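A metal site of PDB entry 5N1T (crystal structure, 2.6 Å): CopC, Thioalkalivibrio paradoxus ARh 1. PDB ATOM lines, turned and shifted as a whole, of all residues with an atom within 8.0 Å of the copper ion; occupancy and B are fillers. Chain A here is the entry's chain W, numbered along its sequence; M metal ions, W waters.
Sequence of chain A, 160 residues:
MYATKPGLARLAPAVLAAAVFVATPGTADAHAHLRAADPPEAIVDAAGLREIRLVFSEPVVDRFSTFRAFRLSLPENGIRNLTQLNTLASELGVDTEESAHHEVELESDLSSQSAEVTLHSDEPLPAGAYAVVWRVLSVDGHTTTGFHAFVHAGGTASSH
N of His 31 lies close to OE1 of Glu 58 (3.0 Å). The side-chain carboxylate (OD1) of Asp 140 lies close to the side-chain hydroxyl (OG) of Ser 138 (3.1 Å).
The copper ion is bound by the side-chain carboxylate (OD2) of Asp 140 (1.9 Å), a ring nitrogen (ND1) of His 142 (2.0 Å), the backbone nitrogen (N) of His 31 (2.0 Å) and a ring nitrogen (ND1) of His 31 (2.0 Å).
Of the 11 residues printed, 3 come within 4 Å of the copper ion.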
ATOM      1  N   HIS A  31      -2.749  29.684 -15.757  1.00  0.00           N
ATOM      2  CA  HIS A  31      -1.459  30.334 -16.172  1.00  0.00           C
ATOM      3  C   HIS A  31      -0.514  30.547 -15.010  1.00  0.00           C
ATOM      4  O   HIS A  31      -0.890  31.091 -13.963  1.00  0.00           O
ATOM      5  CB  HIS A  31      -1.736  31.643 -16.929  1.00  0.00           C
ATOM      6  CG  HIS A  31      -2.372  31.433 -18.269  1.00  0.00           C
ATOM      7  ND1 HIS A  31      -3.506  30.650 -18.457  1.00  0.00           N
ATOM      8  CD2 HIS A  31      -2.019  31.876 -19.506  1.00  0.00           C
ATOM      9  CE1 HIS A  31      -3.821  30.641 -19.741  1.00  0.00           C
ATOM     10  NE2 HIS A  31      -2.942  31.382 -20.394  1.00  0.00           N
ATOM     11  N   ALA A  32       0.706  30.055 -15.169  1.00  0.00           N
ATOM     12  CA  ALA A  32       1.728  30.193 -14.145  1.00  0.00           C
ATOM     13  C   ALA A  32       2.573  31.477 -14.355  1.00  0.00           C
ATOM     14  O   ALA A  32       3.548  31.474 -15.117  1.00  0.00           O
ATOM     15  CB  ALA A  32       2.589  28.943 -14.111  1.00  0.00           C
ATOM     16  N   HIS A  33       2.189  32.568 -13.698  1.00  0.00           N
ATOM     17  CA  HIS A  33       2.905  33.853 -13.789  1.00  0.00           C
ATOM     18  C   HIS A  33       3.886  34.074 -12.620  1.00  0.00           C
ATOM     19  O   HIS A  33       3.646  33.564 -11.515  1.00  0.00           O
ATOM     20  CB  HIS A  33       1.922  35.015 -13.846  1.00  0.00           C
ATOM     21  CG  HIS A  33       0.987  34.953 -15.019  1.00  0.00           C
ATOM     22  ND1 HIS A  33       1.417  35.104 -16.322  1.00  0.00           N
ATOM     23  CD2 HIS A  33      -0.357  34.776 -15.086  1.00  0.00           C
ATOM     24  CE1 HIS A  33       0.377  35.013 -17.141  1.00  0.00           C
ATOM     25  NE2 HIS A  33      -0.703  34.814 -16.412  1.00  0.00           N
ATOM     26  N   GLU A  58       0.899  29.888  -9.762  1.00  0.00           N
ATOM     27  CA  GLU A  58       0.360  28.534  -9.669  1.00  0.00           C
ATOM     28  C   GLU A  58       1.550  27.578  -9.604  1.00  0.00           C
ATOM     29  O   GLU A  58       2.676  27.985  -9.935  1.00  0.00           O
ATOM     30  CB  GLU A  58      -0.476  28.208 -10.897  1.00  0.00           C
ATOM     31  CG  GLU A  58      -1.841  28.864 -10.903  1.00  0.00           C
ATOM     32  CD  GLU A  58      -2.498  28.805 -12.263  1.00  0.00           C
ATOM     33  OE1 GLU A  58      -1.835  28.411 -13.249  1.00  0.00           O
ATOM     34  OE2 GLU A  58      -3.694  29.151 -12.367  1.00  0.00           O
ATOM     35  N   SER A 138       1.892  24.985 -16.333  1.00  0.00           N
ATOM     36  CA  SER A 138       1.115  25.078 -15.115  1.00  0.00           C
ATOM     37  C   SER A 138       0.398  23.754 -14.805  1.00  0.00           C
ATOM     38  O   SER A 138       0.295  22.888 -15.673  1.00  0.00           O
ATOM     39  CB  SER A 138       0.121  26.233 -15.211  1.00  0.00           C
ATOM     40  OG  SER A 138      -0.639  26.313 -14.011  1.00  0.00           O
ATOM     41  N   VAL A 139      -0.071  23.603 -13.563  1.00  0.00           N
ATOM     42  CA  VAL A 139      -0.920  22.442 -13.210  1.00  0.00           C
ATOM     43  C   VAL A 139      -2.319  22.573 -13.817  1.00  0.00           C
ATOM     44  O   VAL A 139      -2.983  21.557 -14.040  1.00  0.00           O
ATOM     45  CB  VAL A 139      -0.942  22.061 -11.681  1.00  0.00           C
ATOM     46  CG1 VAL A 139       0.388  21.452 -11.261  1.00  0.00           C
ATOM     47  CG2 VAL A 139      -1.332  23.238 -10.777  1.00  0.00           C
ATOM     48  N   ASP A 140      -2.717  23.811 -14.113  1.00  0.00           N
ATOM     49  CA  ASP A 140      -3.942  24.121 -14.849  1.00  0.00           C
ATOM     50  C   ASP A 140      -3.831  23.693 -16.333  1.00  0.00           C
ATOM     51  O   ASP A 140      -4.794  23.822 -17.091  1.00  0.00           O
ATOM     52  CB  ASP A 140      -4.317  25.629 -14.691  1.00  0.00           C
ATOM     53  CG  ASP A 140      -3.660  26.563 -15.763  1.00  0.00           C
ATOM     54  OD1 ASP A 140      -2.644  26.194 -16.395  1.00  0.00           O
ATOM     55  OD2 ASP A 140      -4.179  27.684 -15.981  1.00  0.00           O
ATOM     56  N   GLY A 141      -2.647  23.222 -16.746  1.00  0.00           N
ATOM     57  CA  GLY A 141      -2.444  22.699 -18.104  1.00  0.00           C
ATOM     58  C   GLY A 141      -1.867  23.660 -19.128  1.00  0.00           C
ATOM     59  O   GLY A 141      -1.458  23.239 -20.210  1.00  0.00           O
ATOM     60  N   HIS A 142      -1.831  24.941 -18.767  1.00  0.00           N
ATOM     61  CA  HIS A 142      -1.327  25.986 -19.657  1.00  0.00           C
ATOM     62  C   HIS A 142       0.209  26.188 -19.676  1.00  0.00           C
ATOM     63  O   HIS A 142       0.893  26.095 -18.638  1.00  0.00           O
ATOM     64  CB  HIS A 142      -2.069  27.290 -19.398  1.00  0.00           C
ATOM     65  CG  HIS A 142      -3.552  27.170 -19.600  1.00  0.00           C
ATOM     66  ND1 HIS A 142      -4.469  27.808 -18.787  1.00  0.00           N
ATOM     67  CD2 HIS A 142      -4.280  26.490 -20.516  1.00  0.00           C
ATOM     68  CE1 HIS A 142      -5.696  27.532 -19.205  1.00  0.00           C
ATOM     69  NE2 HIS A 142      -5.604  26.729 -20.253  1.00  0.00           N
ATOM     70  N   THR A 143       0.724  26.454 -20.880  1.00  0.00           N
ATOM     71  CA  THR A 143       2.123  26.785 -21.097  1.00  0.00           C
ATOM     72  C   THR A 143       2.229  28.302 -21.178  1.00  0.00           C
ATOM     73  O   THR A 143       1.452  28.955 -21.880  1.00  0.00           O
ATOM     74  CB  THR A 143       2.706  26.096 -22.361  1.00  0.00           C
ATOM     75  OG1 THR A 143       2.800  24.697 -22.112  1.00  0.00           O
ATOM     76  CG2 THR A 143       4.125  26.556 -22.686  1.00  0.00           C
ATOM     77  N   THR A 144       3.156  28.857 -20.421  1.00  0.00           N
ATOM     78  CA  THR A 144       3.558  30.242 -20.539  1.00  0.00           C
ATOM     79  C   THR A 144       5.077  30.345 -20.728  1.00  0.00           C
ATOM     80  O   THR A 144       5.843  29.410 -20.425  1.00  0.00           O
ATOM     81  CB  THR A 144       3.081  31.090 -19.344  1.00  0.00           C
ATOM     82  OG1 THR A 144       3.323  30.380 -18.108  1.00  0.00           O
ATOM     83  CG2 THR A 144       1.606  31.434 -19.498  1.00  0.00           C
HETATM   84 CU    CU M   1      -3.778  28.991 -17.334  1.00  0.00          CU
HETATM   85  O   HOH W   1      -5.316  29.620 -14.523  1.00  0.00           O
